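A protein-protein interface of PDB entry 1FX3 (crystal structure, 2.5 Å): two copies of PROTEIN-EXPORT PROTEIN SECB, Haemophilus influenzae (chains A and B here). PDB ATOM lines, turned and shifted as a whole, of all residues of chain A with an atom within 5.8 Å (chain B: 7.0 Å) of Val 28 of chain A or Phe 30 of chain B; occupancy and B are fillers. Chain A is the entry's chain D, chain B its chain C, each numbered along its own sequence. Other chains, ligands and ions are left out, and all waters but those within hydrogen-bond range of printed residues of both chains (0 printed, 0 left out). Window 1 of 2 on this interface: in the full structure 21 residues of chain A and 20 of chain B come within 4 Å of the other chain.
O of Val 28 of chain B sits at hydrogen-bond distance from N of Phe 30 of chain A, at 3.1 Å. The backbone NH of Phe 30 of chain B sits at hydrogen-bond distance from the backbone carbonyl oxygen of Val 28 of chain A. N of Ala 32 of chain B sits at hydrogen-bond distance from O of Lys 26 of chain A (3.0 Å). The backbone carbonyl oxygen of Leu 35 of chain B lies within hydrogen-bond range of the side-chain amino group of Lys 26 of chain A (3.1 Å). The backbone NH (N) of Val 25 of chain A lies within hydrogen-bond range of the backbone carbonyl oxygen (O) of Arg 129 of chain B (2.9 Å). The side-chain carboxylate of Asp 27 of chain A sits close to the backbone carbonyl oxygen of Phe 30 of chain B (3.5 Å).
The backbone carbonyl oxygen (O) of Ser 29 of chain B sits close to the side-chain sulfur (SG) of Cys 85 of chain B (3.5 Å). The backbone NH of Ser 29 of chain B is in hydrogen-bond range of the backbone carbonyl oxygen of Glu 86 of chain B. O of Glu 31 of chain B sits at hydrogen-bond distance from N of Ile 84 of chain B (2.9 Å). The guanidinium group of Arg 129 of chain B is in hydrogen-bond range of the side-chain amide oxygen of Asn 125 of chain B (2.8 Å). The backbone NH (N) of Lys 26 of chain A is in hydrogen-bond range of the backbone carbonyl oxygen (O) of Lys 88 of chain A (2.9 Å). The backbone carbonyl oxygen (O) of Ser 29 of chain A is in hydrogen-bond range of the backbone NH (N) of Glu 86 of chain A, at 3.1 Å.
O of Val 25 of chain A touches CB of Ala 32 of chain B (3.99 Å). Val 25 of chain A touches Leu 35 of chain B. O of Lys 26 of chain A touches CA of Glu 31 of chain B, at 3.8 Å. Asp 27 of chain A touches Glu 31 of chain B. CA of Ser 29 of chain B touches O of Val 28 of chain A, at 3.4 Å. Val 28 of chain B touches Ser 29 of chain A (O to CA, 3.5 Å). Arg 129 of chain B touches Leu 122 of chain A (NH1 to CD1, 3.4 Å).
Of chain B, only Ser 29 (3.4 Å) and Phe 30 (2.8 Å) come within 4 Å of Val 28 of chain A. Of the printed residues of chain A, Phe 30 of chain B touches Asp 27 and Val 28. Of the printed residues of chain B, Ser 29 of chain A touches Val 28. Of the printed residues of chain A, Ser 29 of chain B touches Val 28. Val 87 of chain A touches none of the printed residues of chain B. The nearest residue of chain A that does not touch Phe 30 of chain B is Val 25 of chain A (4.2 Å). The nearest printed residue of chain B that does not touch Lys 26 of chain A is Phe 30 of chain B (4.3 Å).
Printed residues of chain A that touch a printed residue of chain B: Val 25, Lys 26, Asp 27, Val 28, Ser 29, Phe 30 and Leu 122. Hydrophobic or aromatic side chains of chain A that line the printed part of chain B: Val 25, Val 28, Phe 30 and Leu 122. Among the printed residues, no Asp or Glu carboxylate lies within 4 Å of a Lys or Arg side-chain nitrogen of the other chain.
Val 28 of chain A touches Ser 29 of chain B, and with the chains exchanged Ser 29 of chain A touches Val 28 of chain B. Val 28 of chain A touches Phe 30 of chain B, and with the chains exchanged Phe 30 of chain A touches Val 28 of chain B.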
ATOM      1  N   VAL A  25     -14.160 -26.489   7.508  1.00  0.00           N
ATOM      2  CA  VAL A  25     -14.436 -25.541   8.564  1.00  0.00           C
ATOM      3  C   VAL A  25     -13.258 -25.280   9.510  1.00  0.00           C
ATOM      4  O   VAL A  25     -12.617 -26.210   9.956  1.00  0.00           O
ATOM      5  CB  VAL A  25     -15.634 -26.058   9.330  1.00  0.00           C
ATOM      6  CG1 VAL A  25     -15.733 -25.388  10.701  1.00  0.00           C
ATOM      7  CG2 VAL A  25     -16.886 -25.815   8.459  1.00  0.00           C
ATOM      8  N   LYS A  26     -12.946 -24.020   9.797  1.00  0.00           N
ATOM      9  CA  LYS A  26     -11.846 -23.720  10.726  1.00  0.00           C
ATOM     10  C   LYS A  26     -12.410 -23.504  12.124  1.00  0.00           C
ATOM     11  O   LYS A  26     -11.723 -23.721  13.117  1.00  0.00           O
ATOM     12  CB  LYS A  26     -11.090 -22.444  10.338  1.00  0.00           C
ATOM     13  CG  LYS A  26     -10.328 -22.506   9.027  1.00  0.00           C
ATOM     14  CD  LYS A  26      -9.866 -21.118   8.576  1.00  0.00           C
ATOM     15  CE  LYS A  26      -8.589 -20.661   9.274  1.00  0.00           C
ATOM     16  NZ  LYS A  26      -7.427 -21.502   8.890  1.00  0.00           N
ATOM     17  N   ASP A  27     -13.659 -23.061  12.202  1.00  0.00           N
ATOM     18  CA  ASP A  27     -14.290 -22.786  13.488  1.00  0.00           C
ATOM     19  C   ASP A  27     -15.798 -22.640  13.364  1.00  0.00           C
ATOM     20  O   ASP A  27     -16.298 -22.119  12.378  1.00  0.00           O
ATOM     21  CB  ASP A  27     -13.732 -21.507  14.110  1.00  0.00           C
ATOM     22  CG  ASP A  27     -14.084 -21.389  15.588  1.00  0.00           C
ATOM     23  OD1 ASP A  27     -15.257 -21.652  15.937  1.00  0.00           O
ATOM     24  OD2 ASP A  27     -13.197 -21.040  16.400  1.00  0.00           O
ATOM     25  N   VAL A  28     -16.517 -23.094  14.382  1.00  0.00           N
ATOM     26  CA  VAL A  28     -17.965 -23.029  14.374  1.00  0.00           C
ATOM     27  C   VAL A  28     -18.476 -23.037  15.803  1.00  0.00           C
ATOM     28  O   VAL A  28     -17.965 -23.770  16.647  1.00  0.00           O
ATOM     29  CB  VAL A  28     -18.580 -24.221  13.557  1.00  0.00           C
ATOM     30  CG1 VAL A  28     -17.712 -25.420  13.658  1.00  0.00           C
ATOM     31  CG2 VAL A  28     -19.929 -24.579  14.083  1.00  0.00           C
ATOM     32  N   SER A  29     -19.471 -22.192  16.060  1.00  0.00           N
ATOM     33  CA  SER A  29     -20.094 -22.058  17.375  1.00  0.00           C
ATOM     34  C   SER A  29     -21.600 -21.852  17.207  1.00  0.00           C
ATOM     35  O   SER A  29     -22.054 -21.367  16.174  1.00  0.00           O
ATOM     36  CB  SER A  29     -19.512 -20.862  18.091  1.00  0.00           C
ATOM     37  OG  SER A  29     -19.925 -19.696  17.431  1.00  0.00           O
ATOM     38  N   PHE A  30     -22.377 -22.237  18.212  1.00  0.00           N
ATOM     39  CA  PHE A  30     -23.820 -22.071  18.153  1.00  0.00           C
ATOM     40  C   PHE A  30     -24.439 -22.195  19.517  1.00  0.00           C
ATOM     41  O   PHE A  30     -24.803 -23.294  19.932  1.00  0.00           O
ATOM     42  CB  PHE A  30     -24.454 -23.113  17.267  1.00  0.00           C
ATOM     43  CG  PHE A  30     -25.958 -23.118  17.318  1.00  0.00           C
ATOM     44  CD1 PHE A  30     -26.695 -22.350  16.430  1.00  0.00           C
ATOM     45  CD2 PHE A  30     -26.633 -23.961  18.187  1.00  0.00           C
ATOM     46  CE1 PHE A  30     -28.079 -22.434  16.398  1.00  0.00           C
ATOM     47  CE2 PHE A  30     -28.011 -24.052  18.165  1.00  0.00           C
ATOM     48  CZ  PHE A  30     -28.739 -23.289  17.264  1.00  0.00           C
ATOM     49  N   GLU A  86     -21.651 -18.672  14.766  1.00  0.00           N
ATOM     50  CA  GLU A  86     -20.468 -18.045  14.215  1.00  0.00           C
ATOM     51  C   GLU A  86     -19.614 -19.073  13.506  1.00  0.00           C
ATOM     52  O   GLU A  86     -18.880 -19.852  14.115  1.00  0.00           O
ATOM     53  CB  GLU A  86     -19.673 -17.335  15.302  1.00  0.00           C
ATOM     54  CG  GLU A  86     -20.181 -15.938  15.603  1.00  0.00           C
ATOM     55  CD  GLU A  86     -19.169 -15.109  16.383  1.00  0.00           C
ATOM     56  OE1 GLU A  86     -18.004 -15.012  15.930  1.00  0.00           O
ATOM     57  OE2 GLU A  86     -19.537 -14.549  17.442  1.00  0.00           O
ATOM     58  N   VAL A  87     -19.707 -19.024  12.189  1.00  0.00           N
ATOM     59  CA  VAL A  87     -19.031 -19.936  11.299  1.00  0.00           C
ATOM     60  C   VAL A  87     -17.830 -19.400  10.537  1.00  0.00           C
ATOM     61  O   VAL A  87     -17.801 -18.259  10.094  1.00  0.00           O
ATOM     62  CB  VAL A  87     -20.054 -20.453  10.284  1.00  0.00           C
ATOM     63  CG1 VAL A  87     -19.375 -20.940   9.032  1.00  0.00           C
ATOM     64  CG2 VAL A  87     -20.879 -21.542  10.916  1.00  0.00           C
ATOM     65  N   LYS A  88     -16.823 -20.241  10.406  1.00  0.00           N
ATOM     66  CA  LYS A  88     -15.658 -19.907   9.615  1.00  0.00           C
ATOM     67  C   LYS A  88     -15.564 -21.039   8.598  1.00  0.00           C
ATOM     68  O   LYS A  88     -14.982 -22.096   8.883  1.00  0.00           O
ATOM     69  CB  LYS A  88     -14.388 -19.855  10.453  1.00  0.00           C
ATOM     70  CG  LYS A  88     -14.128 -18.515  11.092  1.00  0.00           C
ATOM     71  CD  LYS A  88     -12.663 -18.414  11.500  1.00  0.00           C
ATOM     72  CE  LYS A  88     -12.292 -17.028  11.988  1.00  0.00           C
ATOM     73  NZ  LYS A  88     -10.821 -16.939  12.232  1.00  0.00           N
ATOM     74  N   LEU A 122     -24.542 -25.178   6.664  1.00  0.00           N
ATOM     75  CA  LEU A 122     -23.957 -25.403   7.970  1.00  0.00           C
ATOM     76  C   LEU A 122     -24.883 -24.672   8.934  1.00  0.00           C
ATOM     77  O   LEU A 122     -25.485 -25.306   9.803  1.00  0.00           O
ATOM     78  CB  LEU A 122     -22.531 -24.850   8.068  1.00  0.00           C
ATOM     79  CG  LEU A 122     -21.921 -24.905   9.481  1.00  0.00           C
ATOM     80  CD1 LEU A 122     -21.950 -26.320  10.035  1.00  0.00           C
ATOM     81  CD2 LEU A 122     -20.495 -24.402   9.424  1.00  0.00           C
ATOM     82  N   LEU A 126     -27.158 -26.411  12.055  1.00  0.00           N
ATOM     83  CA  LEU A 126     -27.036 -26.100  13.476  1.00  0.00           C
ATOM     84  C   LEU A 126     -28.398 -25.644  13.979  1.00  0.00           C
ATOM     85  O   LEU A 126     -29.020 -26.324  14.797  1.00  0.00           O
ATOM     86  CB  LEU A 126     -25.998 -25.001  13.696  1.00  0.00           C
ATOM     87  CG  LEU A 126     -24.629 -25.529  13.263  1.00  0.00           C
ATOM     88  CD1 LEU A 126     -23.652 -24.403  13.026  1.00  0.00           C
ATOM     89  CD2 LEU A 126     -24.119 -26.521  14.329  1.00  0.00           C
ATOM     90  N   VAL B  28     -22.738 -25.830  21.174  1.00  0.00           N
ATOM     91  CA  VAL B  28     -21.838 -26.670  20.413  1.00  0.00           C
ATOM     92  C   VAL B  28     -20.740 -25.811  19.878  1.00  0.00           C
ATOM     93  O   VAL B  28     -20.977 -24.703  19.431  1.00  0.00           O
ATOM     94  CB  VAL B  28     -22.561 -27.402  19.218  1.00  0.00           C
ATOM     95  CG1 VAL B  28     -23.805 -26.688  18.836  1.00  0.00           C
ATOM     96  CG2 VAL B  28     -21.650 -27.492  18.015  1.00  0.00           C
ATOM     97  N   SER B  29     -19.525 -26.331  19.937  1.00  0.00           N
ATOM     98  CA  SER B  29     -18.369 -25.617  19.430  1.00  0.00           C
ATOM     99  C   SER B  29     -17.361 -26.561  18.778  1.00  0.00           C
ATOM    100  O   SER B  29     -17.129 -27.677  19.253  1.00  0.00           O
ATOM    101  CB  SER B  29     -17.711 -24.859  20.563  1.00  0.00           C
ATOM    102  OG  SER B  29     -16.312 -25.026  20.528  1.00  0.00           O
ATOM    103  N   PHE B  30     -16.776 -26.111  17.672  1.00  0.00           N
ATOM    104  CA  PHE B  30     -15.781 -26.902  16.963  1.00  0.00           C
ATOM    105  C   PHE B  30     -14.685 -25.985  16.456  1.00  0.00           C
ATOM    106  O   PHE B  30     -14.943 -25.091  15.653  1.00  0.00           O
ATOM    107  CB  PHE B  30     -16.416 -27.630  15.786  1.00  0.00           C
ATOM    108  CG  PHE B  30     -15.438 -28.425  14.977  1.00  0.00           C
ATOM    109  CD1 PHE B  30     -15.247 -29.782  15.222  1.00  0.00           C
ATOM    110  CD2 PHE B  30     -14.670 -27.806  13.999  1.00  0.00           C
ATOM    111  CE1 PHE B  30     -14.304 -30.501  14.503  1.00  0.00           C
ATOM    112  CE2 PHE B  30     -13.725 -28.515  13.279  1.00  0.00           C
ATOM    113  CZ  PHE B  30     -13.539 -29.863  13.528  1.00  0.00           C
ATOM    114  N   GLU B  31     -13.457 -26.225  16.911  1.00  0.00           N
ATOM    115  CA  GLU B  31     -12.309 -25.416  16.523  1.00  0.00           C
ATOM    116  C   GLU B  31     -11.170 -26.281  15.985  1.00  0.00           C
ATOM    117  O   GLU B  31     -10.776 -27.268  16.612  1.00  0.00           O
ATOM    118  CB  GLU B  31     -11.834 -24.614  17.726  1.00  0.00           C
ATOM    119  CG  GLU B  31     -10.604 -23.755  17.485  1.00  0.00           C
ATOM    120  CD  GLU B  31      -9.978 -23.268  18.789  1.00  0.00           C
ATOM    121  OE1 GLU B  31      -8.874 -22.670  18.733  1.00  0.00           O
ATOM    122  OE2 GLU B  31     -10.593 -23.486  19.865  1.00  0.00           O
ATOM    123  N   ALA B  32     -10.655 -25.892  14.816  1.00  0.00           N
ATOM    124  CA  ALA B  32      -9.558 -26.576  14.115  1.00  0.00           C
ATOM    125  C   ALA B  32      -8.542 -25.488  13.772  1.00  0.00           C
ATOM    126  O   ALA B  32      -8.474 -24.995  12.646  1.00  0.00           O
ATOM    127  CB  ALA B  32     -10.069 -27.241  12.847  1.00  0.00           C
ATOM    128  N   PRO B  33      -7.728 -25.123  14.756  1.00  0.00           N
ATOM    129  CA  PRO B  33      -6.662 -24.124  14.811  1.00  0.00           C
ATOM    130  C   PRO B  33      -5.419 -24.198  13.938  1.00  0.00           C
ATOM    131  O   PRO B  33      -4.747 -23.188  13.757  1.00  0.00           O
ATOM    132  CB  PRO B  33      -6.292 -24.132  16.288  1.00  0.00           C
ATOM    133  CG  PRO B  33      -6.439 -25.558  16.628  1.00  0.00           C
ATOM    134  CD  PRO B  33      -7.780 -25.866  16.028  1.00  0.00           C
ATOM    135  N   LEU B  35      -5.229 -25.374  10.646  1.00  0.00           N
ATOM    136  CA  LEU B  35      -5.606 -25.635   9.275  1.00  0.00           C
ATOM    137  C   LEU B  35      -5.022 -24.565   8.350  1.00  0.00           C
ATOM    138  O   LEU B  35      -4.957 -23.388   8.701  1.00  0.00           O
ATOM    139  CB  LEU B  35      -7.119 -25.653   9.186  1.00  0.00           C
ATOM    140  CG  LEU B  35      -7.738 -27.033   9.361  1.00  0.00           C
ATOM    141  CD1 LEU B  35      -7.089 -27.782  10.490  1.00  0.00           C
ATOM    142  CD2 LEU B  35      -9.213 -26.865   9.587  1.00  0.00           C
ATOM    143  N   ALA B  82      -5.489 -31.030  16.333  1.00  0.00           N
ATOM    144  CA  ALA B  82      -6.198 -31.194  15.082  1.00  0.00           C
ATOM    145  C   ALA B  82      -7.594 -30.539  15.205  1.00  0.00           C
ATOM    146  O   ALA B  82      -8.044 -29.803  14.322  1.00  0.00           O
ATOM    147  CB  ALA B  82      -6.320 -32.681  14.738  1.00  0.00           C
ATOM    148  N   PHE B  83      -8.278 -30.822  16.302  1.00  0.00           N
ATOM    149  CA  PHE B  83      -9.583 -30.247  16.539  1.00  0.00           C
ATOM    150  C   PHE B  83      -9.993 -30.431  17.980  1.00  0.00           C
ATOM    151  O   PHE B  83      -9.546 -31.379  18.645  1.00  0.00           O
ATOM    152  CB  PHE B  83     -10.643 -30.883  15.614  1.00  0.00           C
ATOM    153  CG  PHE B  83     -10.898 -32.340  15.867  1.00  0.00           C
ATOM    154  CD1 PHE B  83     -11.621 -32.760  16.981  1.00  0.00           C
ATOM    155  CD2 PHE B  83     -10.437 -33.304  14.967  1.00  0.00           C
ATOM    156  CE1 PHE B  83     -11.890 -34.139  17.201  1.00  0.00           C
ATOM    157  CE2 PHE B  83     -10.700 -34.674  15.170  1.00  0.00           C
ATOM    158  CZ  PHE B  83     -11.431 -35.099  16.290  1.00  0.00           C
ATOM    159  N   ILE B  84     -10.814 -29.493  18.455  1.00  0.00           N
ATOM    160  CA  ILE B  84     -11.382 -29.511  19.796  1.00  0.00           C
ATOM    161  C   ILE B  84     -12.849 -29.338  19.511  1.00  0.00           C
ATOM    162  O   ILE B  84     -13.233 -28.527  18.675  1.00  0.00           O
ATOM    163  CB  ILE B  84     -10.921 -28.328  20.671  1.00  0.00           C
ATOM    164  CG1 ILE B  84      -9.469 -28.517  21.081  1.00  0.00           C
ATOM    165  CG2 ILE B  84     -11.736 -28.288  21.951  1.00  0.00           C
ATOM    166  CD1 ILE B  84      -8.943 -27.433  21.986  1.00  0.00           C
ATOM    167  N   CYS B  85     -13.686 -30.107  20.179  1.00  0.00           N
ATOM    168  CA  CYS B  85     -15.095 -29.995  19.920  1.00  0.00           C
ATOM    169  C   CYS B  85     -15.835 -30.217  21.217  1.00  0.00           C
ATOM    170  O   CYS B  85     -15.530 -31.143  21.960  1.00  0.00           O
ATOM    171  CB  CYS B  85     -15.510 -31.015  18.862  1.00  0.00           C
ATOM    172  SG  CYS B  85     -17.268 -31.036  18.459  1.00  0.00           S
ATOM    173  N   GLU B  86     -16.812 -29.354  21.480  1.00  0.00           N
ATOM    174  CA  GLU B  86     -17.579 -29.434  22.698  1.00  0.00           C
ATOM    175  C   GLU B  86     -19.035 -29.343  22.329  1.00  0.00           C
ATOM    176  O   GLU B  86     -19.420 -28.524  21.516  1.00  0.00           O
ATOM    177  CB  GLU B  86     -17.160 -28.295  23.630  1.00  0.00           C
ATOM    178  CG  GLU B  86     -15.637 -28.178  23.761  1.00  0.00           C
ATOM    179  CD  GLU B  86     -15.161 -27.511  25.059  1.00  0.00           C
ATOM    180  OE1 GLU B  86     -15.850 -27.647  26.096  1.00  0.00           O
ATOM    181  OE2 GLU B  86     -14.079 -26.874  25.043  1.00  0.00           O
ATOM    182  N   LEU B 122     -23.617 -35.277  16.203  1.00  0.00           N
ATOM    183  CA  LEU B 122     -23.121 -33.917  16.026  1.00  0.00           C
ATOM    184  C   LEU B 122     -21.579 -33.880  15.933  1.00  0.00           C
ATOM    185  O   LEU B 122     -21.009 -33.176  15.090  1.00  0.00           O
ATOM    186  CB  LEU B 122     -23.645 -32.998  17.146  1.00  0.00           C
ATOM    187  CG  LEU B 122     -23.065 -31.573  17.294  1.00  0.00           C
ATOM    188  CD1 LEU B 122     -23.036 -30.879  15.977  1.00  0.00           C
ATOM    189  CD2 LEU B 122     -23.896 -30.762  18.265  1.00  0.00           C
ATOM    190  N   VAL B 123     -20.901 -34.651  16.782  1.00  0.00           N
ATOM    191  CA  VAL B 123     -19.444 -34.657  16.763  1.00  0.00           C
ATOM    192  C   VAL B 123     -18.936 -35.215  15.432  1.00  0.00           C
ATOM    193  O   VAL B 123     -18.122 -34.578  14.771  1.00  0.00           O
ATOM    194  CB  VAL B 123     -18.859 -35.494  17.924  1.00  0.00           C
ATOM    195  CG1 VAL B 123     -17.307 -35.632  17.763  1.00  0.00           C
ATOM    196  CG2 VAL B 123     -19.196 -34.821  19.254  1.00  0.00           C
ATOM    197  N   ASN B 125     -20.384 -35.287  12.695  1.00  0.00           N
ATOM    198  CA  ASN B 125     -20.753 -34.323  11.666  1.00  0.00           C
ATOM    199  C   ASN B 125     -19.743 -33.177  11.581  1.00  0.00           C
ATOM    200  O   ASN B 125     -19.273 -32.812  10.502  1.00  0.00           O
ATOM    201  CB  ASN B 125     -22.159 -33.788  11.944  1.00  0.00           C
ATOM    202  CG  ASN B 125     -22.850 -33.257  10.690  1.00  0.00           C
ATOM    203  OD1 ASN B 125     -22.513 -32.197  10.173  1.00  0.00           O
ATOM    204  ND2 ASN B 125     -23.829 -34.002  10.207  1.00  0.00           N
ATOM    205  N   LEU B 126     -19.377 -32.617  12.715  1.00  0.00           N
ATOM    206  CA  LEU B 126     -18.411 -31.528  12.681  1.00  0.00           C
ATOM    207  C   LEU B 126     -16.958 -31.956  12.382  1.00  0.00           C
ATOM    208  O   LEU B 126     -16.261 -31.254  11.645  1.00  0.00           O
ATOM    209  CB  LEU B 126     -18.472 -30.742  13.994  1.00  0.00           C
ATOM    210  CG  LEU B 126     -19.837 -30.065  14.255  1.00  0.00           C
ATOM    211  CD1 LEU B 126     -19.994 -29.777  15.719  1.00  0.00           C
ATOM    212  CD2 LEU B 126     -19.953 -28.782  13.453  1.00  0.00           C
ATOM    213  N   VAL B 127     -16.484 -33.082  12.928  1.00  0.00           N
ATOM    214  CA  VAL B 127     -15.115 -33.452  12.638  1.00  0.00           C
ATOM    215  C   VAL B 127     -15.086 -33.666  11.136  1.00  0.00           C
ATOM    216  O   VAL B 127     -14.100 -33.322  10.484  1.00  0.00           O
ATOM    217  CB  VAL B 127     -14.601 -34.756  13.372  1.00  0.00           C
ATOM    218  CG1 VAL B 127     -14.845 -34.666  14.854  1.00  0.00           C
ATOM    219  CG2 VAL B 127     -15.226 -35.971  12.808  1.00  0.00           C
ATOM    220  N   ASN B 128     -16.176 -34.188  10.571  1.00  0.00           N
ATOM    221  CA  ASN B 128     -16.178 -34.398   9.132  1.00  0.00           C
ATOM    222  C   ASN B 128     -16.141 -33.114   8.306  1.00  0.00           C
ATOM    223  O   ASN B 128     -15.659 -33.152   7.185  1.00  0.00           O
ATOM    224  CB  ASN B 128     -17.351 -35.272   8.698  1.00  0.00           C
ATOM    225  CG  ASN B 128     -17.387 -35.490   7.204  1.00  0.00           C
ATOM    226  OD1 ASN B 128     -18.196 -34.867   6.494  1.00  0.00           O
ATOM    227  ND2 ASN B 128     -16.517 -36.378   6.711  1.00  0.00           N
ATOM    228  N   ARG B 129     -16.609 -31.982   8.842  1.00  0.00           N
ATOM    229  CA  ARG B 129     -16.575 -30.723   8.082  1.00  0.00           C
ATOM    230  C   ARG B 129     -15.188 -30.165   8.145  1.00  0.00           C
ATOM    231  O   ARG B 129     -14.837 -29.260   7.402  1.00  0.00           O
ATOM    232  CB  ARG B 129     -17.555 -29.688   8.637  1.00  0.00           C
ATOM    233  CG  ARG B 129     -19.005 -30.101   8.413  1.00  0.00           C
ATOM    234  CD  ARG B 129     -19.958 -29.358   9.335  1.00  0.00           C
ATOM    235  NE  ARG B 129     -21.324 -29.858   9.185  1.00  0.00           N
ATOM    236  CZ  ARG B 129     -22.189 -29.426   8.272  1.00  0.00           C
ATOM    237  NH1 ARG B 129     -21.835 -28.473   7.422  1.00  0.00           N
ATOM    238  NH2 ARG B 129     -23.401 -29.949   8.206  1.00  0.00           N
ATOM    239  N   GLY B 130     -14.400 -30.687   9.071  1.00  0.00           N
ATOM    240  CA  GLY B 130     -13.021 -30.248   9.158  1.00  0.00           C
ATOM    241  C   GLY B 130     -12.194 -31.162   8.254  1.00  0.00           C
ATOM    242  O   GLY B 130     -10.986 -31.005   8.145  1.00  0.00           O
ATOM    243  N   THR B 131     -12.867 -32.119   7.615  1.00  0.00           N
ATOM    244  CA  THR B 131     -12.253 -33.081   6.703  1.00  0.00           C
ATOM    245  C   THR B 131     -11.199 -33.933   7.398  1.00  0.00           C
ATOM    246  O   THR B 131     -10.143 -34.197   6.837  1.00  0.00           O
ATOM    247  CB  THR B 131     -11.595 -32.392   5.448  1.00  0.00           C
ATOM    248  OG1 THR B 131     -10.549 -31.504   5.874  1.00  0.00           O
ATOM    249  CG2 THR B 131     -12.629 -31.595   4.650  1.00  0.00           C
ATOM    250  N   PHE B 132     -11.470 -34.337   8.634  1.00  0.00           N
ATOM    251  CA  PHE B 132     -10.546 -35.195   9.338  1.00  0.00           C
ATOM    252  C   PHE B 132     -11.149 -36.586   9.328  1.00  0.00           C
ATOM    253  O   PHE B 132     -12.332 -36.754   9.109  1.00  0.00           O
ATOM    254  CB  PHE B 132     -10.383 -34.770  10.791  1.00  0.00           C
ATOM    255  CG  PHE B 132      -9.860 -33.387  10.976  1.00  0.00           C
ATOM    256  CD1 PHE B 132     -10.690 -32.374  11.432  1.00  0.00           C
ATOM    257  CD2 PHE B 132      -8.526 -33.101  10.747  1.00  0.00           C
ATOM    258  CE1 PHE B 132     -10.189 -31.098  11.663  1.00  0.00           C
ATOM    259  CE2 PHE B 132      -8.019 -31.829  10.971  1.00  0.00           C
ATOM    260  CZ  PHE B 132      -8.848 -30.828  11.431  1.00  0.00           C
